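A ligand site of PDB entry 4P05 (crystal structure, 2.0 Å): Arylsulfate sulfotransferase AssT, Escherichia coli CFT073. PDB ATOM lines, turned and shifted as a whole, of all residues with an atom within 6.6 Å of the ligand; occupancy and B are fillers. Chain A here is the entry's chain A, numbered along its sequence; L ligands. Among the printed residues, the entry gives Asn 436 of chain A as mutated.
The side-chain hydroxyl (OH) of Tyr 208 lies within hydrogen-bond range of an oxygen (O1) of the ligand, at 3.1 Å.
NE2 of His 356 sits at hydrogen-bond distance from O3 of the ligand (2.9 Å).
ND2 of Asn 358 sits at hydrogen-bond distance from O4 of the ligand (2.8 Å).
An oxygen (O6) of the ligand is in hydrogen-bond range of the backbone NH (N) of Thr 501, 2.9 Å away.
A ring nitrogen (NE2) of His 252 sits at hydrogen-bond distance from an oxygen (O3) of the ligand (3.1 Å).
An oxygen (O6) of the ligand lies within salt-bridge range of the guanidinium group (NE) of Arg 374 (3.7 Å).
The side-chain amide oxygen (OD1) of Asn 436 sits close to an oxygen (O4) of the ligand, at 3.3 Å.
OD1 of Asn 451 lies within hydrogen-bond range of ND2 of Asn 436 (3.0 Å).
ND2 of Asn 358 sits at hydrogen-bond distance from O of Gln 435.
The side-chain amide nitrogen of Asn 358 sits close to the side-chain amide nitrogen of Asn 436, at 3.5 Å.
NH2 of Arg 374 sits at hydrogen-bond distance from O of Pro 499.
The backbone carbonyl oxygen (O) of Thr 501 sits close to the side-chain amide nitrogen (ND2) of Asn 436, 3.1 Å away.
The backbone NH (N) of His 252 sits at hydrogen-bond distance from the side-chain sulfur (SD) of Met 210 (3.2 Å).
The backbone carbonyl oxygen of Ile 500 sits at hydrogen-bond distance from the side-chain hydroxyl of Ser 502 (3.0 Å).
OH of Tyr 559 lies within hydrogen-bond range of O of His 252 (2.7 Å).
Residues that only touch the ligand: Thr 557, Ile 500, Tyr 559 and Phe 171.
Hydrophobic or aromatic side chains within 4 Å of the ligand: Phe 171, Tyr 208, His 252, His 356, Ile 500 and Tyr 559.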
ATOM      1  N   PHE A 171     -18.484   9.316  10.963  1.00  0.00           N
ATOM      2  CA  PHE A 171     -18.028   8.005  11.291  1.00  0.00           C
ATOM      3  C   PHE A 171     -17.410   7.324  10.082  1.00  0.00           C
ATOM      4  O   PHE A 171     -17.983   6.440   9.457  1.00  0.00           O
ATOM      5  CB  PHE A 171     -19.208   7.178  11.756  1.00  0.00           C
ATOM      6  CG  PHE A 171     -18.869   5.992  12.619  1.00  0.00           C
ATOM      7  CD1 PHE A 171     -18.163   6.158  13.769  1.00  0.00           C
ATOM      8  CD2 PHE A 171     -19.382   4.735  12.337  1.00  0.00           C
ATOM      9  CE1 PHE A 171     -17.898   5.102  14.607  1.00  0.00           C
ATOM     10  CE2 PHE A 171     -19.100   3.651  13.147  1.00  0.00           C
ATOM     11  CZ  PHE A 171     -18.367   3.827  14.305  1.00  0.00           C
ATOM     12  N   ILE A 173     -13.470   6.288   8.249  1.00  0.00           N
ATOM     13  CA  ILE A 173     -12.067   5.959   8.474  1.00  0.00           C
ATOM     14  C   ILE A 173     -11.544   4.928   7.461  1.00  0.00           C
ATOM     15  O   ILE A 173     -12.317   4.048   6.933  1.00  0.00           O
ATOM     16  CB  ILE A 173     -11.908   5.493   9.935  1.00  0.00           C
ATOM     17  CG1 ILE A 173     -10.469   5.411  10.386  1.00  0.00           C
ATOM     18  CG2 ILE A 173     -12.568   4.154  10.172  1.00  0.00           C
ATOM     19  CD1 ILE A 173     -10.375   5.033  11.870  1.00  0.00           C
ATOM     20  N   TYR A 208     -17.197   3.412   7.227  1.00  0.00           N
ATOM     21  CA  TYR A 208     -16.437   2.632   8.161  1.00  0.00           C
ATOM     22  C   TYR A 208     -16.634   1.172   7.816  1.00  0.00           C
ATOM     23  O   TYR A 208     -17.639   0.586   8.172  1.00  0.00           O
ATOM     24  CB  TYR A 208     -16.902   2.972   9.560  1.00  0.00           C
ATOM     25  CG  TYR A 208     -15.943   2.678  10.692  1.00  0.00           C
ATOM     26  CD1 TYR A 208     -15.296   1.448  10.798  1.00  0.00           C
ATOM     27  CD2 TYR A 208     -15.722   3.639  11.709  1.00  0.00           C
ATOM     28  CE1 TYR A 208     -14.408   1.191  11.862  1.00  0.00           C
ATOM     29  CE2 TYR A 208     -14.840   3.387  12.778  1.00  0.00           C
ATOM     30  CZ  TYR A 208     -14.173   2.153  12.858  1.00  0.00           C
ATOM     31  OH  TYR A 208     -13.342   1.874  13.943  1.00  0.00           O
ATOM     32  N   MET A 210     -17.120  -2.399   7.993  1.00  0.00           N
ATOM     33  CA  MET A 210     -17.434  -3.186   9.129  1.00  0.00           C
ATOM     34  C   MET A 210     -18.422  -4.252   8.758  1.00  0.00           C
ATOM     35  O   MET A 210     -18.999  -4.239   7.700  1.00  0.00           O
ATOM     36  CB  MET A 210     -18.193  -2.377  10.174  1.00  0.00           C
ATOM     37  CG  MET A 210     -17.455  -1.158  10.664  1.00  0.00           C
ATOM     38  SD  MET A 210     -18.564  -0.043  11.486  1.00  0.00           S
ATOM     39  CE  MET A 210     -18.073  -0.135  13.194  1.00  0.00           C
ATOM     40  N   HIS A 252     -21.434  -1.551  11.581  1.00  0.00           N
ATOM     41  CA  HIS A 252     -21.375  -2.649  12.621  1.00  0.00           C
ATOM     42  C   HIS A 252     -21.617  -4.060  12.156  1.00  0.00           C
ATOM     43  O   HIS A 252     -20.878  -5.017  12.613  1.00  0.00           O
ATOM     44  CB  HIS A 252     -22.238  -2.350  13.851  1.00  0.00           C
ATOM     45  CG  HIS A 252     -21.685  -1.222  14.654  1.00  0.00           C
ATOM     46  ND1 HIS A 252     -21.977   0.093  14.400  1.00  0.00           N
ATOM     47  CD2 HIS A 252     -20.787  -1.197  15.639  1.00  0.00           C
ATOM     48  CE1 HIS A 252     -21.298   0.873  15.216  1.00  0.00           C
ATOM     49  NE2 HIS A 252     -20.568   0.098  15.977  1.00  0.00           N
ATOM     50  N   ARG A 283     -28.207   4.530  14.398  1.00  0.00           N
ATOM     51  CA  ARG A 283     -27.976   3.154  14.815  1.00  0.00           C
ATOM     52  C   ARG A 283     -29.142   2.502  15.435  1.00  0.00           C
ATOM     53  O   ARG A 283     -28.976   1.688  16.333  1.00  0.00           O
ATOM     54  CB  ARG A 283     -26.754   3.053  15.733  1.00  0.00           C
ATOM     55  CG  ARG A 283     -25.469   3.526  15.075  1.00  0.00           C
ATOM     56  CD  ARG A 283     -24.186   3.326  15.900  1.00  0.00           C
ATOM     57  NE  ARG A 283     -23.187   4.141  15.273  1.00  0.00           N
ATOM     58  CZ  ARG A 283     -22.819   5.339  15.665  1.00  0.00           C
ATOM     59  NH1 ARG A 283     -21.959   5.988  14.919  1.00  0.00           N
ATOM     60  NH2 ARG A 283     -23.251   5.886  16.787  1.00  0.00           N
ATOM     61  N   ALA A 320     -15.088   6.977  25.357  1.00  0.00           N
ATOM     62  CA  ALA A 320     -15.522   6.021  24.289  1.00  0.00           C
ATOM     63  C   ALA A 320     -16.943   6.286  23.749  1.00  0.00           C
ATOM     64  O   ALA A 320     -17.213   6.209  22.531  1.00  0.00           O
ATOM     65  CB  ALA A 320     -15.414   4.593  24.802  1.00  0.00           C
ATOM     66  N   HIS A 356     -27.477   2.459  19.865  1.00  0.00           N
ATOM     67  CA  HIS A 356     -26.259   2.029  19.334  1.00  0.00           C
ATOM     68  C   HIS A 356     -26.292   0.565  19.146  1.00  0.00           C
ATOM     69  O   HIS A 356     -25.438  -0.164  19.725  1.00  0.00           O
ATOM     70  CB  HIS A 356     -25.169   2.430  20.295  1.00  0.00           C
ATOM     71  CG  HIS A 356     -23.796   2.358  19.726  1.00  0.00           C
ATOM     72  ND1 HIS A 356     -23.054   3.492  19.446  1.00  0.00           N
ATOM     73  CD2 HIS A 356     -23.030   1.298  19.383  1.00  0.00           C
ATOM     74  CE1 HIS A 356     -21.893   3.130  18.929  1.00  0.00           C
ATOM     75  NE2 HIS A 356     -21.864   1.806  18.858  1.00  0.00           N
ATOM     76  N   VAL A 357     -27.193   0.079  18.299  1.00  0.00           N
ATOM     77  CA  VAL A 357     -27.240  -1.351  18.005  1.00  0.00           C
ATOM     78  C   VAL A 357     -26.001  -1.755  17.199  1.00  0.00           C
ATOM     79  O   VAL A 357     -25.564  -1.004  16.290  1.00  0.00           O
ATOM     80  CB  VAL A 357     -28.518  -1.740  17.280  1.00  0.00           C
ATOM     81  CG1 VAL A 357     -28.418  -3.145  16.760  1.00  0.00           C
ATOM     82  CG2 VAL A 357     -29.759  -1.668  18.163  1.00  0.00           C
ATOM     83  N   ASN A 358     -25.410  -2.898  17.527  1.00  0.00           N
ATOM     84  CA  ASN A 358     -24.119  -3.282  17.029  1.00  0.00           C
ATOM     85  C   ASN A 358     -23.893  -4.698  16.642  1.00  0.00           C
ATOM     86  O   ASN A 358     -22.832  -5.067  16.153  1.00  0.00           O
ATOM     87  CB  ASN A 358     -23.006  -2.808  17.951  1.00  0.00           C
ATOM     88  CG  ASN A 358     -23.029  -3.397  19.330  1.00  0.00           C
ATOM     89  OD1 ASN A 358     -23.604  -4.458  19.571  1.00  0.00           O
ATOM     90  ND2 ASN A 358     -22.332  -2.733  20.258  1.00  0.00           N
ATOM     91  N   ARG A 374     -25.859  -1.549  22.366  1.00  0.00           N
ATOM     92  CA  ARG A 374     -24.808  -1.190  23.297  1.00  0.00           C
ATOM     93  C   ARG A 374     -25.336  -0.405  24.525  1.00  0.00           C
ATOM     94  O   ARG A 374     -24.809  -0.545  25.617  1.00  0.00           O
ATOM     95  CB  ARG A 374     -23.751  -0.382  22.618  1.00  0.00           C
ATOM     96  CG  ARG A 374     -22.460  -0.183  23.423  1.00  0.00           C
ATOM     97  CD  ARG A 374     -21.529   0.854  22.784  1.00  0.00           C
ATOM     98  NE  ARG A 374     -20.243   0.965  23.479  1.00  0.00           N
ATOM     99  CZ  ARG A 374     -19.937   1.876  24.370  1.00  0.00           C
ATOM    100  NH1 ARG A 374     -20.801   2.784  24.727  1.00  0.00           N
ATOM    101  NH2 ARG A 374     -18.762   1.820  24.965  1.00  0.00           N
ATOM    102  N   THR A 434     -22.669  -2.564  27.651  1.00  0.00           N
ATOM    103  CA  THR A 434     -22.071  -2.118  26.425  1.00  0.00           C
ATOM    104  C   THR A 434     -21.571  -3.236  25.557  1.00  0.00           C
ATOM    105  O   THR A 434     -20.534  -3.147  24.898  1.00  0.00           O
ATOM    106  CB  THR A 434     -20.955  -1.051  26.698  1.00  0.00           C
ATOM    107  OG1 THR A 434     -19.971  -1.652  27.529  1.00  0.00           O
ATOM    108  CG2 THR A 434     -21.539   0.129  27.402  1.00  0.00           C
ATOM    109  N   GLN A 435     -22.319  -4.335  25.519  1.00  0.00           N
ATOM    110  CA  GLN A 435     -21.852  -5.469  24.828  1.00  0.00           C
ATOM    111  C   GLN A 435     -21.783  -5.373  23.271  1.00  0.00           C
ATOM    112  O   GLN A 435     -22.340  -4.435  22.654  1.00  0.00           O
ATOM    113  CB  GLN A 435     -22.669  -6.658  25.268  1.00  0.00           C
ATOM    114  CG  GLN A 435     -24.036  -6.716  24.720  1.00  0.00           C
ATOM    115  CD  GLN A 435     -24.915  -5.607  25.171  1.00  0.00           C
ATOM    116  OE1 GLN A 435     -24.970  -5.253  26.336  1.00  0.00           O
ATOM    117  NE2 GLN A 435     -25.632  -5.026  24.233  1.00  0.00           N
ATOM    118  N   ASN A 436     -21.124  -6.364  22.673  1.00  0.00           N
ATOM    119  CA  ASN A 436     -20.975  -6.554  21.255  1.00  0.00           C
ATOM    120  C   ASN A 436     -21.315  -8.003  20.849  1.00  0.00           C
ATOM    121  O   ASN A 436     -21.306  -8.900  21.643  1.00  0.00           O
ATOM    122  CB  ASN A 436     -19.595  -6.191  20.782  1.00  0.00           C
ATOM    123  CG  ASN A 436     -19.399  -4.666  20.509  1.00  0.00           C
ATOM    124  OD1 ASN A 436     -19.300  -4.256  19.388  1.00  0.00           O
ATOM    125  ND2 ASN A 436     -19.328  -3.870  21.560  1.00  0.00           N
ATOM    126  N   ASN A 451     -18.195  -6.291  26.819  1.00  0.00           N
ATOM    127  CA  ASN A 451     -17.167  -5.220  26.922  1.00  0.00           C
ATOM    128  C   ASN A 451     -16.926  -4.714  28.342  1.00  0.00           C
ATOM    129  O   ASN A 451     -15.754  -4.615  28.772  1.00  0.00           O
ATOM    130  CB  ASN A 451     -17.509  -4.029  26.013  1.00  0.00           C
ATOM    131  CG  ASN A 451     -17.520  -4.449  24.564  1.00  0.00           C
ATOM    132  OD1 ASN A 451     -18.429  -5.178  24.116  1.00  0.00           O
ATOM    133  ND2 ASN A 451     -16.462  -4.064  23.811  1.00  0.00           N
ATOM    134  N   PRO A 499     -13.185  -1.651  25.873  1.00  0.00           N
ATOM    135  CA  PRO A 499     -14.363  -0.852  26.079  1.00  0.00           C
ATOM    136  C   PRO A 499     -15.340  -0.822  24.851  1.00  0.00           C
ATOM    137  O   PRO A 499     -16.595  -0.714  24.998  1.00  0.00           O
ATOM    138  CB  PRO A 499     -13.806   0.555  26.298  1.00  0.00           C
ATOM    139  CG  PRO A 499     -12.451   0.560  25.656  1.00  0.00           C
ATOM    140  CD  PRO A 499     -11.956  -0.843  25.747  1.00  0.00           C
ATOM    141  N   ILE A 500     -14.773  -0.923  23.659  1.00  0.00           N
ATOM    142  CA  ILE A 500     -15.586  -0.948  22.447  1.00  0.00           C
ATOM    143  C   ILE A 500     -15.259  -2.097  21.518  1.00  0.00           C
ATOM    144  O   ILE A 500     -14.279  -2.834  21.709  1.00  0.00           O
ATOM    145  CB  ILE A 500     -15.500   0.414  21.684  1.00  0.00           C
ATOM    146  CG1 ILE A 500     -14.077   0.684  21.275  1.00  0.00           C
ATOM    147  CG2 ILE A 500     -16.111   1.554  22.521  1.00  0.00           C
ATOM    148  CD1 ILE A 500     -13.778   2.034  20.588  1.00  0.00           C
ATOM    149  N   THR A 501     -16.117  -2.243  20.509  1.00  0.00           N
ATOM    150  CA  THR A 501     -15.937  -3.164  19.427  1.00  0.00           C
ATOM    151  C   THR A 501     -15.827  -4.605  19.936  1.00  0.00           C
ATOM    152  O   THR A 501     -16.448  -4.893  20.951  1.00  0.00           O
ATOM    153  CB  THR A 501     -14.822  -2.785  18.453  1.00  0.00           C
ATOM    154  OG1 THR A 501     -13.571  -3.199  18.933  1.00  0.00           O
ATOM    155  CG2 THR A 501     -14.745  -1.306  18.202  1.00  0.00           C
ATOM    156  N   SER A 502     -15.043  -5.448  19.269  1.00  0.00           N
ATOM    157  CA  SER A 502     -14.752  -6.823  19.743  1.00  0.00           C
ATOM    158  C   SER A 502     -15.784  -7.871  19.393  1.00  0.00           C
ATOM    159  O   SER A 502     -16.868  -7.572  18.988  1.00  0.00           O
ATOM    160  CB  SER A 502     -14.455  -6.890  21.256  1.00  0.00           C
ATOM    161  OG  SER A 502     -13.643  -5.757  21.585  1.00  0.00           O
ATOM    162  N   LEU A 522      -6.905   1.254  24.725  1.00  0.00           N
ATOM    163  CA  LEU A 522      -7.327   2.389  23.895  1.00  0.00           C
ATOM    164  C   LEU A 522      -6.974   3.702  24.535  1.00  0.00           C
ATOM    165  O   LEU A 522      -6.515   4.641  23.815  1.00  0.00           O
ATOM    166  CB  LEU A 522      -8.806   2.375  23.611  1.00  0.00           C
ATOM    167  CG  LEU A 522      -9.437   3.401  22.634  1.00  0.00           C
ATOM    168  CD1 LEU A 522      -8.862   3.290  21.240  1.00  0.00           C
ATOM    169  CD2 LEU A 522     -10.930   3.124  22.628  1.00  0.00           C
ATOM    170  N   THR A 557      -8.734   2.272  17.509  1.00  0.00           N
ATOM    171  CA  THR A 557      -9.353   1.006  17.768  1.00  0.00           C
ATOM    172  C   THR A 557      -9.360   0.016  16.568  1.00  0.00           C
ATOM    173  O   THR A 557      -9.324   0.416  15.451  1.00  0.00           O
ATOM    174  CB  THR A 557     -10.758   1.253  18.305  1.00  0.00           C
ATOM    175  OG1 THR A 557     -11.308   0.029  18.854  1.00  0.00           O
ATOM    176  CG2 THR A 557     -11.691   1.734  17.128  1.00  0.00           C
ATOM    177  N   HIS A 558      -9.403  -1.283  16.828  1.00  0.00           N
ATOM    178  CA  HIS A 558      -9.623  -2.330  15.855  1.00  0.00           C
ATOM    179  C   HIS A 558     -11.100  -2.623  15.993  1.00  0.00           C
ATOM    180  O   HIS A 558     -11.726  -2.135  16.906  1.00  0.00           O
ATOM    181  CB  HIS A 558      -8.807  -3.647  16.125  1.00  0.00           C
ATOM    182  CG  HIS A 558      -7.329  -3.414  16.339  1.00  0.00           C
ATOM    183  ND1 HIS A 558      -6.468  -3.124  15.311  1.00  0.00           N
ATOM    184  CD2 HIS A 558      -6.605  -3.238  17.467  1.00  0.00           C
ATOM    185  CE1 HIS A 558      -5.279  -2.818  15.778  1.00  0.00           C
ATOM    186  NE2 HIS A 558      -5.335  -2.888  17.088  1.00  0.00           N
ATOM    187  N   TYR A 559     -11.698  -3.278  15.037  1.00  0.00           N
ATOM    188  CA  TYR A 559     -13.135  -3.495  15.138  1.00  0.00           C
ATOM    189  C   TYR A 559     -13.371  -5.011  15.463  1.00  0.00           C
ATOM    190  O   TYR A 559     -13.842  -5.360  16.538  1.00  0.00           O
ATOM    191  CB  TYR A 559     -13.932  -3.018  13.859  1.00  0.00           C
ATOM    192  CG  TYR A 559     -15.402  -3.269  13.988  1.00  0.00           C
ATOM    193  CD1 TYR A 559     -16.086  -2.707  15.000  1.00  0.00           C
ATOM    194  CD2 TYR A 559     -16.079  -4.148  13.153  1.00  0.00           C
ATOM    195  CE1 TYR A 559     -17.425  -2.979  15.221  1.00  0.00           C
ATOM    196  CE2 TYR A 559     -17.413  -4.440  13.343  1.00  0.00           C
ATOM    197  CZ  TYR A 559     -18.106  -3.866  14.388  1.00  0.00           C
ATOM    198  OH  TYR A 559     -19.426  -4.147  14.679  1.00  0.00           O
HETATM  199  O1  LIG L   1     -14.080   3.492  16.427  1.00  0.00           O
HETATM  200  N1  LIG L   1     -14.839   3.958  17.265  1.00  0.00           N
HETATM  201  O2  LIG L   1     -14.741   5.278  17.797  1.00  0.00           O
HETATM  202  C1  LIG L   1     -15.900   3.164  17.646  1.00  0.00           C
HETATM  203  C2  LIG L   1     -16.167   2.075  16.855  1.00  0.00           C
HETATM  204  C3  LIG L   1     -17.236   1.284  17.169  1.00  0.00           C
HETATM  205  C4  LIG L   1     -16.652   3.561  18.687  1.00  0.00           C
HETATM  206  C5  LIG L   1     -17.709   2.757  19.027  1.00  0.00           C
HETATM  207  C6  LIG L   1     -17.987   1.644  18.263  1.00  0.00           C
HETATM  208  O3  LIG L   1     -19.087   0.945  18.601  1.00  0.00           O
HETATM  209  S1  LIG L   1     -19.039  -0.522  19.037  1.00  0.00           S
HETATM  210  O4  LIG L   1     -20.309  -1.160  19.196  1.00  0.00           O
HETATM  211  O5  LIG L   1     -18.255  -1.238  18.125  1.00  0.00           O
HETATM  212  O6  LIG L   1     -18.475  -0.477  20.527  1.00  0.00           O
